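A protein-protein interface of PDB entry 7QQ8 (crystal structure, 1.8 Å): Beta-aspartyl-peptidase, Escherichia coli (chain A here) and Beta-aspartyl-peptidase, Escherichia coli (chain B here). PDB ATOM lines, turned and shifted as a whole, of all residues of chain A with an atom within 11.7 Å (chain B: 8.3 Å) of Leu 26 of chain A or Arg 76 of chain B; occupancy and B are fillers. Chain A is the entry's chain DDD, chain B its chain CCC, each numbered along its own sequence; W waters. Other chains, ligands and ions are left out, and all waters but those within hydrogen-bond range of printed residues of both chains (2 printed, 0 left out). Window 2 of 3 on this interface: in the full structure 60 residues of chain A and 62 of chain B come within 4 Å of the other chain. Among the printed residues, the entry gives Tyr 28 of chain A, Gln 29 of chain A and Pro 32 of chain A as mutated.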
ATOM      1  N   THR A  19     -24.402   1.481 -10.939  1.00  0.00           N
ATOM      2  CA  THR A  19     -24.773   2.769 -10.341  1.00  0.00           C
ATOM      3  C   THR A  19     -25.477   3.655 -11.374  1.00  0.00           C
ATOM      4  O   THR A  19     -25.421   3.366 -12.562  1.00  0.00           O
ATOM      5  CB  THR A  19     -23.548   3.509  -9.779  1.00  0.00           C
ATOM      6  OG1 THR A  19     -24.020   4.596  -8.976  1.00  0.00           O
ATOM      7  CG2 THR A  19     -22.637   4.041 -10.848  1.00  0.00           C
ATOM      8  N   GLY A  20     -26.173   4.687 -10.865  1.00  0.00           N
ATOM      9  CA  GLY A  20     -26.554   5.849 -11.675  1.00  0.00           C
ATOM     10  C   GLY A  20     -25.675   7.036 -11.347  1.00  0.00           C
ATOM     11  O   GLY A  20     -25.884   8.068 -11.951  1.00  0.00           O
ATOM     12  N   GLY A  21     -24.685   6.889 -10.456  1.00  0.00           N
ATOM     13  CA  GLY A  21     -23.723   7.978 -10.192  1.00  0.00           C
ATOM     14  C   GLY A  21     -24.228   8.963  -9.147  1.00  0.00           C
ATOM     15  O   GLY A  21     -24.992   8.540  -8.301  1.00  0.00           O
ATOM     16  N   MET A  22     -23.763  10.221  -9.148  1.00  0.00           N
ATOM     17  CA  MET A  22     -24.134  11.257  -8.141  1.00  0.00           C
ATOM     18  C   MET A  22     -25.339  12.021  -8.659  1.00  0.00           C
ATOM     19  O   MET A  22     -25.333  12.352  -9.878  1.00  0.00           O
ATOM     20  CB  MET A  22     -23.033  12.302  -7.950  1.00  0.00           C
ATOM     21  CG  MET A  22     -21.702  11.711  -7.596  1.00  0.00           C
ATOM     22  SD  MET A  22     -20.293  12.869  -7.702  1.00  0.00           S
ATOM     23  CE  MET A  22     -20.888  14.131  -8.834  1.00  0.00           C
ATOM     24  N   THR A  23     -26.276  12.384  -7.782  1.00  0.00           N
ATOM     25  CA  THR A  23     -27.421  13.252  -8.175  1.00  0.00           C
ATOM     26  C   THR A  23     -26.819  14.509  -8.824  1.00  0.00           C
ATOM     27  O   THR A  23     -25.773  14.944  -8.356  1.00  0.00           O
ATOM     28  CB  THR A  23     -28.394  13.550  -7.021  1.00  0.00           C
ATOM     29  OG1 THR A  23     -29.176  12.385  -6.764  1.00  0.00           O
ATOM     30  CG2 THR A  23     -29.372  14.668  -7.308  1.00  0.00           C
ATOM     31  N   ASN A  24     -27.419  14.976  -9.915  1.00  0.00           N
ATOM     32  CA  ASN A  24     -27.104  16.267 -10.564  1.00  0.00           C
ATOM     33  C   ASN A  24     -25.742  16.168 -11.272  1.00  0.00           C
ATOM     34  O   ASN A  24     -25.107  17.235 -11.497  1.00  0.00           O
ATOM     35  CB  ASN A  24     -27.116  17.396  -9.525  1.00  0.00           C
ATOM     36  CG  ASN A  24     -27.455  18.752 -10.112  1.00  0.00           C
ATOM     37  OD1 ASN A  24     -28.236  18.845 -11.064  1.00  0.00           O
ATOM     38  ND2 ASN A  24     -26.932  19.812  -9.505  1.00  0.00           N
ATOM     39  N   LYS A  25     -25.260  14.964 -11.590  1.00  0.00           N
ATOM     40  CA  LYS A  25     -23.919  14.833 -12.211  1.00  0.00           C
ATOM     41  C   LYS A  25     -23.980  15.440 -13.619  1.00  0.00           C
ATOM     42  O   LYS A  25     -25.057  15.432 -14.261  1.00  0.00           O
ATOM     43  CB  LYS A  25     -23.438  13.379 -12.249  1.00  0.00           C
ATOM     44  CG  LYS A  25     -24.245  12.471 -13.156  1.00  0.00           C
ATOM     45  CD  LYS A  25     -23.739  11.060 -13.175  1.00  0.00           C
ATOM     46  CE  LYS A  25     -24.607  10.139 -13.995  1.00  0.00           C
ATOM     47  NZ  LYS A  25     -23.948   8.814 -14.170  1.00  0.00           N
ATOM     48  N   LEU A  26     -22.832  15.905 -14.106  1.00  0.00           N
ATOM     49  CA  LEU A  26     -22.640  16.149 -15.550  1.00  0.00           C
ATOM     50  C   LEU A  26     -22.863  14.837 -16.286  1.00  0.00           C
ATOM     51  O   LEU A  26     -22.364  13.792 -15.862  1.00  0.00           O
ATOM     52  CB  LEU A  26     -21.227  16.664 -15.810  1.00  0.00           C
ATOM     53  CG  LEU A  26     -20.962  18.114 -15.435  1.00  0.00           C
ATOM     54  CD1 LEU A  26     -19.484  18.403 -15.654  1.00  0.00           C
ATOM     55  CD2 LEU A  26     -21.839  19.090 -16.222  1.00  0.00           C
ATOM     56  N   PRO A  27     -23.601  14.888 -17.412  1.00  0.00           N
ATOM     57  CA  PRO A  27     -23.603  13.791 -18.363  1.00  0.00           C
ATOM     58  C   PRO A  27     -22.151  13.521 -18.804  1.00  0.00           C
ATOM     59  O   PRO A  27     -21.388  14.474 -18.884  1.00  0.00           O
ATOM     60  CB  PRO A  27     -24.505  14.276 -19.520  1.00  0.00           C
ATOM     61  CG  PRO A  27     -24.714  15.767 -19.303  1.00  0.00           C
ATOM     62  CD  PRO A  27     -24.435  16.016 -17.839  1.00  0.00           C
ATOM     63  N   TYR A  28     -21.798  12.247 -19.017  1.00  0.00           N
ATOM     64  CA  TYR A  28     -20.481  11.807 -19.563  1.00  0.00           C
ATOM     65  C   TYR A  28     -19.367  11.944 -18.492  1.00  0.00           C
ATOM     66  O   TYR A  28     -18.103  12.057 -18.835  1.00  0.00           O
ATOM     67  CB  TYR A  28     -20.115  12.635 -20.804  1.00  0.00           C
ATOM     68  CG  TYR A  28     -21.034  12.598 -22.012  1.00  0.00           C
ATOM     69  CD1 TYR A  28     -21.026  11.528 -22.890  1.00  0.00           C
ATOM     70  CD2 TYR A  28     -21.814  13.690 -22.362  1.00  0.00           C
ATOM     71  CE1 TYR A  28     -21.808  11.512 -24.032  1.00  0.00           C
ATOM     72  CE2 TYR A  28     -22.604  13.698 -23.501  1.00  0.00           C
ATOM     73  CZ  TYR A  28     -22.606  12.599 -24.343  1.00  0.00           C
ATOM     74  OH  TYR A  28     -23.365  12.574 -25.485  1.00  0.00           O
ATOM     75  N   GLN A  29     -19.766  12.071 -17.218  1.00  0.00           N
ATOM     76  CA  GLN A  29     -18.813  11.909 -16.093  1.00  0.00           C
ATOM     77  C   GLN A  29     -18.790  10.420 -15.735  1.00  0.00           C
ATOM     78  O   GLN A  29     -19.861   9.796 -15.783  1.00  0.00           O
ATOM     79  CB  GLN A  29     -19.165  12.791 -14.897  1.00  0.00           C
ATOM     80  CG  GLN A  29     -18.003  12.930 -13.928  1.00  0.00           C
ATOM     81  CD  GLN A  29     -18.123  12.062 -12.694  1.00  0.00           C
ATOM     82  OE1 GLN A  29     -19.161  12.039 -12.027  1.00  0.00           O
ATOM     83  NE2 GLN A  29     -17.039  11.370 -12.362  1.00  0.00           N
ATOM     84  N   VAL A  30     -17.596   9.876 -15.511  1.00  0.00           N
ATOM     85  CA  VAL A  30     -17.372   8.437 -15.202  1.00  0.00           C
ATOM     86  C   VAL A  30     -16.743   8.323 -13.809  1.00  0.00           C
ATOM     87  O   VAL A  30     -15.521   8.655 -13.637  1.00  0.00           O
ATOM     88  CB  VAL A  30     -16.460   7.725 -16.204  1.00  0.00           C
ATOM     89  CG1 VAL A  30     -16.512   6.233 -15.963  1.00  0.00           C
ATOM     90  CG2 VAL A  30     -16.794   8.050 -17.646  1.00  0.00           C
ATOM     91  N   GLY A  31     -17.526   7.804 -12.878  1.00  0.00           N
ATOM     92  CA  GLY A  31     -17.089   7.506 -11.507  1.00  0.00           C
ATOM     93  C   GLY A  31     -16.413   6.149 -11.480  1.00  0.00           C
ATOM     94  O   GLY A  31     -16.095   5.582 -12.527  1.00  0.00           O
ATOM     95  N   PRO A  32     -16.179   5.620 -10.263  1.00  0.00           N
ATOM     96  CA  PRO A  32     -15.333   4.446 -10.091  1.00  0.00           C
ATOM     97  C   PRO A  32     -16.009   3.172 -10.591  1.00  0.00           C
ATOM     98  O   PRO A  32     -15.335   2.231 -10.900  1.00  0.00           O
ATOM     99  CB  PRO A  32     -15.103   4.350  -8.568  1.00  0.00           C
ATOM    100  CG  PRO A  32     -16.207   5.168  -7.958  1.00  0.00           C
ATOM    101  CD  PRO A  32     -16.703   6.166  -9.001  1.00  0.00           C
ATOM    102  N   GLU A  56     -14.448  10.192  -7.027  1.00  0.00           N
ATOM    103  CA  GLU A  56     -13.100  10.450  -7.536  1.00  0.00           C
ATOM    104  C   GLU A  56     -12.066   9.807  -6.622  1.00  0.00           C
ATOM    105  O   GLU A  56     -11.124   9.220  -7.118  1.00  0.00           O
ATOM    106  CB  GLU A  56     -13.033  11.956  -7.747  1.00  0.00           C
ATOM    107  CG  GLU A  56     -13.974  12.346  -8.862  1.00  0.00           C
ATOM    108  CD  GLU A  56     -15.469  12.284  -8.617  1.00  0.00           C
ATOM    109  OE1 GLU A  56     -15.887  12.090  -7.460  1.00  0.00           O
ATOM    110  OE2 GLU A  56     -16.215  12.444  -9.591  1.00  0.00           O
ATOM    111  N   VAL B  73     -30.398   7.840  -9.848  1.00  0.00           N
ATOM    112  CA  VAL B  73     -30.438   9.319  -9.640  1.00  0.00           C
ATOM    113  C   VAL B  73     -30.556   9.972 -11.007  1.00  0.00           C
ATOM    114  O   VAL B  73     -30.284   9.313 -12.036  1.00  0.00           O
ATOM    115  CB  VAL B  73     -29.205   9.881  -8.921  1.00  0.00           C
ATOM    116  CG1 VAL B  73     -29.106   9.374  -7.478  1.00  0.00           C
ATOM    117  CG2 VAL B  73     -27.937   9.582  -9.721  1.00  0.00           C
ATOM    118  N   PHE B  74     -30.929  11.236 -10.967  1.00  0.00           N
ATOM    119  CA  PHE B  74     -31.055  12.116 -12.146  1.00  0.00           C
ATOM    120  C   PHE B  74     -29.770  12.932 -12.298  1.00  0.00           C
ATOM    121  O   PHE B  74     -29.233  13.454 -11.288  1.00  0.00           O
ATOM    122  CB  PHE B  74     -32.270  13.023 -11.973  1.00  0.00           C
ATOM    123  CG  PHE B  74     -33.609  12.352 -12.141  1.00  0.00           C
ATOM    124  CD1 PHE B  74     -34.218  11.691 -11.082  1.00  0.00           C
ATOM    125  CD2 PHE B  74     -34.281  12.420 -13.356  1.00  0.00           C
ATOM    126  CE1 PHE B  74     -35.464  11.085 -11.249  1.00  0.00           C
ATOM    127  CE2 PHE B  74     -35.524  11.824 -13.515  1.00  0.00           C
ATOM    128  CZ  PHE B  74     -36.119  11.162 -12.463  1.00  0.00           C
ATOM    129  N   THR B  75     -29.344  13.105 -13.549  1.00  0.00           N
ATOM    130  CA  THR B  75     -28.212  13.970 -13.945  1.00  0.00           C
ATOM    131  C   THR B  75     -28.681  15.425 -13.961  1.00  0.00           C
ATOM    132  O   THR B  75     -29.885  15.661 -13.880  1.00  0.00           O
ATOM    133  CB  THR B  75     -27.705  13.621 -15.350  1.00  0.00           C
ATOM    134  OG1 THR B  75     -28.756  13.915 -16.272  1.00  0.00           O
ATOM    135  CG2 THR B  75     -27.297  12.164 -15.469  1.00  0.00           C
ATOM    136  N   ARG B  76     -27.759  16.342 -14.211  1.00  0.00           N
ATOM    137  CA  ARG B  76     -28.047  17.792 -14.279  1.00  0.00           C
ATOM    138  C   ARG B  76     -29.168  18.011 -15.298  1.00  0.00           C
ATOM    139  O   ARG B  76     -29.947  18.949 -15.130  1.00  0.00           O
ATOM    140  CB  ARG B  76     -26.754  18.519 -14.661  1.00  0.00           C
ATOM    141  CG  ARG B  76     -26.863  20.034 -14.793  1.00  0.00           C
ATOM    142  CD  ARG B  76     -26.516  20.766 -13.505  1.00  0.00           C
ATOM    143  NE  ARG B  76     -25.377  20.174 -12.805  1.00  0.00           N
ATOM    144  CZ  ARG B  76     -24.092  20.440 -13.033  1.00  0.00           C
ATOM    145  NH1 ARG B  76     -23.176  19.819 -12.305  1.00  0.00           N
ATOM    146  NH2 ARG B  76     -23.728  21.318 -13.961  1.00  0.00           N
ATOM    147  N   ASP B  77     -29.246  17.156 -16.325  1.00  0.00           N
ATOM    148  CA  ASP B  77     -30.178  17.318 -17.475  1.00  0.00           C
ATOM    149  C   ASP B  77     -31.463  16.512 -17.228  1.00  0.00           C
ATOM    150  O   ASP B  77     -32.257  16.389 -18.166  1.00  0.00           O
ATOM    151  CB  ASP B  77     -29.513  16.912 -18.797  1.00  0.00           C
ATOM    152  CG  ASP B  77     -28.234  17.673 -19.154  1.00  0.00           C
ATOM    153  OD1 ASP B  77     -27.948  18.757 -18.572  1.00  0.00           O
ATOM    154  OD2 ASP B  77     -27.512  17.179 -20.020  1.00  0.00           O
ATOM    155  N   GLU B  78     -31.679  15.992 -16.014  1.00  0.00           N
ATOM    156  CA  GLU B  78     -32.903  15.226 -15.656  1.00  0.00           C
ATOM    157  C   GLU B  78     -33.003  13.977 -16.517  1.00  0.00           C
ATOM    158  O   GLU B  78     -34.121  13.538 -16.768  1.00  0.00           O
ATOM    159  CB  GLU B  78     -34.170  16.060 -15.808  1.00  0.00           C
ATOM    160  CG  GLU B  78     -34.012  17.440 -15.184  1.00  0.00           C
ATOM    161  CD  GLU B  78     -35.336  18.133 -14.898  1.00  0.00           C
ATOM    162  OE1 GLU B  78     -36.387  17.579 -15.298  1.00  0.00           O
ATOM    163  OE2 GLU B  78     -35.322  19.202 -14.257  1.00  0.00           O
ATOM    164  N   THR B  79     -31.847  13.424 -16.863  1.00  0.00           N
ATOM    165  CA  THR B  79     -31.679  12.131 -17.577  1.00  0.00           C
ATOM    166  C   THR B  79     -31.149  11.090 -16.585  1.00  0.00           C
ATOM    167  O   THR B  79     -30.948  11.428 -15.400  1.00  0.00           O
ATOM    168  CB  THR B  79     -30.724  12.302 -18.770  1.00  0.00           C
ATOM    169  OG1 THR B  79     -29.408  12.643 -18.322  1.00  0.00           O
ATOM    170  CG2 THR B  79     -31.192  13.370 -19.734  1.00  0.00           C
ATOM    171  N   HIS B  80     -30.932   9.869 -17.059  1.00  0.00           N
ATOM    172  CA  HIS B  80     -30.218   8.803 -16.310  1.00  0.00           C
ATOM    173  C   HIS B  80     -29.081   8.298 -17.208  1.00  0.00           C
ATOM    174  O   HIS B  80     -29.325   8.102 -18.435  1.00  0.00           O
ATOM    175  CB  HIS B  80     -31.210   7.703 -15.895  1.00  0.00           C
ATOM    176  CG  HIS B  80     -32.390   8.179 -15.125  1.00  0.00           C
ATOM    177  ND1 HIS B  80     -32.298   8.623 -13.818  1.00  0.00           N
ATOM    178  CD2 HIS B  80     -33.689   8.293 -15.486  1.00  0.00           C
ATOM    179  CE1 HIS B  80     -33.486   8.994 -13.410  1.00  0.00           C
ATOM    180  NE2 HIS B  80     -34.367   8.812 -14.422  1.00  0.00           N
ATOM    181  N   GLU B  81     -27.888   8.192 -16.651  1.00  0.00           N
ATOM    182  CA  GLU B  81     -26.704   7.557 -17.276  1.00  0.00           C
ATOM    183  C   GLU B  81     -26.159   6.536 -16.277  1.00  0.00           C
ATOM    184  O   GLU B  81     -25.810   6.907 -15.130  1.00  0.00           O
ATOM    185  CB  GLU B  81     -25.635   8.603 -17.589  1.00  0.00           C
ATOM    186  CG  GLU B  81     -25.917   9.403 -18.840  1.00  0.00           C
ATOM    187  CD  GLU B  81     -25.071  10.628 -19.135  1.00  0.00           C
ATOM    188  OE1 GLU B  81     -24.015  10.864 -18.474  1.00  0.00           O
ATOM    189  OE2 GLU B  81     -25.493  11.376 -20.075  1.00  0.00           O
ATOM    190  N   LEU B 153     -33.274  15.561  -6.619  1.00  0.00           N
ATOM    191  CA  LEU B 153     -32.662  16.460  -7.641  1.00  0.00           C
ATOM    192  C   LEU B 153     -33.123  17.908  -7.365  1.00  0.00           C
ATOM    193  O   LEU B 153     -32.249  18.805  -7.301  1.00  0.00           O
ATOM    194  CB  LEU B 153     -33.025  15.996  -9.056  1.00  0.00           C
ATOM    195  CG  LEU B 153     -32.541  16.906 -10.192  1.00  0.00           C
ATOM    196  CD1 LEU B 153     -31.029  16.809 -10.391  1.00  0.00           C
ATOM    197  CD2 LEU B 153     -33.278  16.603 -11.498  1.00  0.00           C
ATOM    198  N   ALA B 156     -31.436  19.521  -4.418  1.00  0.00           N
ATOM    199  CA  ALA B 156     -29.997  19.826  -4.635  1.00  0.00           C
ATOM    200  C   ALA B 156     -29.787  21.179  -5.365  1.00  0.00           C
ATOM    201  O   ALA B 156     -28.613  21.614  -5.401  1.00  0.00           O
ATOM    202  CB  ALA B 156     -29.329  18.664  -5.371  1.00  0.00           C
ATOM    203  N   ARG B 157     -30.825  21.827  -5.938  1.00  0.00           N
ATOM    204  CA  ARG B 157     -30.642  22.974  -6.886  1.00  0.00           C
ATOM    205  C   ARG B 157     -31.671  24.107  -6.707  1.00  0.00           C
ATOM    206  O   ARG B 157     -32.722  23.942  -6.103  1.00  0.00           O
ATOM    207  CB  ARG B 157     -30.729  22.440  -8.308  1.00  0.00           C
ATOM    208  CG  ARG B 157     -32.119  21.971  -8.687  1.00  0.00           C
ATOM    209  CD  ARG B 157     -32.010  21.280 -10.022  1.00  0.00           C
ATOM    210  NE  ARG B 157     -33.334  21.030 -10.559  1.00  0.00           N
ATOM    211  CZ  ARG B 157     -33.582  20.511 -11.766  1.00  0.00           C
ATOM    212  NH1 ARG B 157     -32.591  20.176 -12.582  1.00  0.00           N
ATOM    213  NH2 ARG B 157     -34.836  20.330 -12.142  1.00  0.00           N
HETATM  214  O   HOH W   1     -31.715  12.306  -8.268  1.00  0.00           O
HETATM  215  O   HOH W   2     -28.103   8.531 -13.713  1.00  0.00           O
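The backbone carbonyl oxygen (O) of Phe 74 of chain B sits at hydrogen-bond distance from the backbone NH (N) of Asn 24 of chain A (2.7 Å). NE of Arg 76 of chain B sits at hydrogen-bond distance from O of Asn 24 of chain A (3.2 Å). The backbone NH of Arg 76 of chain B is in hydrogen-bond range of the backbone carbonyl oxygen of Lys 25 of chain A, 2.9 Å away. The backbone carbonyl oxygen of Glu 81 of chain B sits at hydrogen-bond distance from the side-chain amino group of Lys 25 of chain A, at 2.8 Å. OE1 of Glu 81 of chain B lies within hydrogen-bond range of N of Tyr 28 of chain A, at 2.7 Å. O of Glu 81 of chain B lies close to O of Gly 20 of chain A, at 3.4 Å.
The backbone carbonyl oxygen of Val 73 of chain B is in hydrogen-bond range of a ring nitrogen (ND1) of His 80 of chain B, 2.8 Å away. The side-chain hydroxyl (OG1) of Thr 75 of chain B sits close to the backbone NH (N) of Asp 77 of chain B (3.3 Å). The side-chain hydroxyl of Thr 75 of chain B sits at hydrogen-bond distance from the side-chain hydroxyl of Thr 79 of chain B. The side-chain hydroxyl (OG1) of Thr 19 of chain A is in hydrogen-bond range of the backbone NH (N) of Gly 21 of chain A (2.8 Å). The backbone carbonyl oxygen (O) of Gly 20 of chain A is in hydrogen-bond range of the side-chain amino group (NZ) of Lys 25 of chain A (3.0 Å).
Among the printed residues, merely in contact across the chains: Pro 27 of chain A with Glu 81 of chain B (3.0 Å), Thr 23 of chain A with Val 73 of chain B (3.1 Å), Pro 27 of chain A with Asp 77 of chain B (3.2 Å), Lys 25 of chain A with Thr 75 of chain B (3.4 Å), Gly 20 of chain A with Val 73 of chain B (3.4 Å), Gly 21 of chain A with Val 73 of chain B (3.4 Å), Asn 24 of chain A with Leu 153 of chain B (3.5 Å), Thr 23 of chain A with Phe 74 of chain B (3.6 Å), Leu 26 of chain A with Arg 76 of chain B (3.7 Å), Met 22 of chain A with Val 73 of chain B (3.7 Å), Thr 23 of chain A with Leu 153 of chain B (3.8 Å) and Asn 24 of chain A with Thr 75 of chain B (3.8 Å).
Of chain B, only Arg 76 comes within 4 Å of Leu 26 of chain A. Thr 75 of chain B touches just these residues of chain A: Asn 24 (3.8 Å) and Lys 25 (3.4 Å). Of chain A, only Pro 27 (3.2 Å) comes within 4 Å of Asp 77 of chain B. No residue of chain A comes within 4 Å of Thr 79 of chain B. Of the printed residues of chain B, Lys 25 of chain A touches Thr 75 (3.4 Å), Arg 76 (2.9 Å) and Glu 81 (2.8 Å). Printed residues of chain B within 4 Å of Met 22 of chain A: Val 73 (3.7 Å). Printed residues of chain B within 4 Å of Tyr 28 of chain A: Glu 81 (2.7 Å). Of the printed residues of chain B, Asn 24 of chain A touches Phe 74, Thr 75, Arg 76 and Leu 153. His 80 of chain B touches none of the printed residues of chain A. The nearest residue of chain B that does not touch Leu 26 of chain A is Glu 81 of chain B (4.3 Å). The nearest residue of chain A that does not touch Arg 76 of chain B is Pro 27 of chain A (4.7 Å).
Of the 12 printed residues of chain B, 7 touch a printed residue of chain A. Printed residues of chain A that touch a printed residue of chain B: Gly 20, Gly 21, Met 22, Thr 23, Asn 24, Lys 25, Leu 26, Pro 27 and Tyr 28. Along chain A the printed residues that touch a printed residue of chain B span positions 20 to 28. Among the printed residues, 18 pairs touch across the chains.
Water W2 lies within hydrogen-bond range of O of Val 73 of chain B (2.9 Å), O of Gly 20 of chain A (2.9 Å) and N of Glu 81 of chain B (3.0 Å). Water W1 bridges OG1 of Thr 23 of chain A (3.0 Å) and N of Phe 74 of chain B (3.0 Å).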
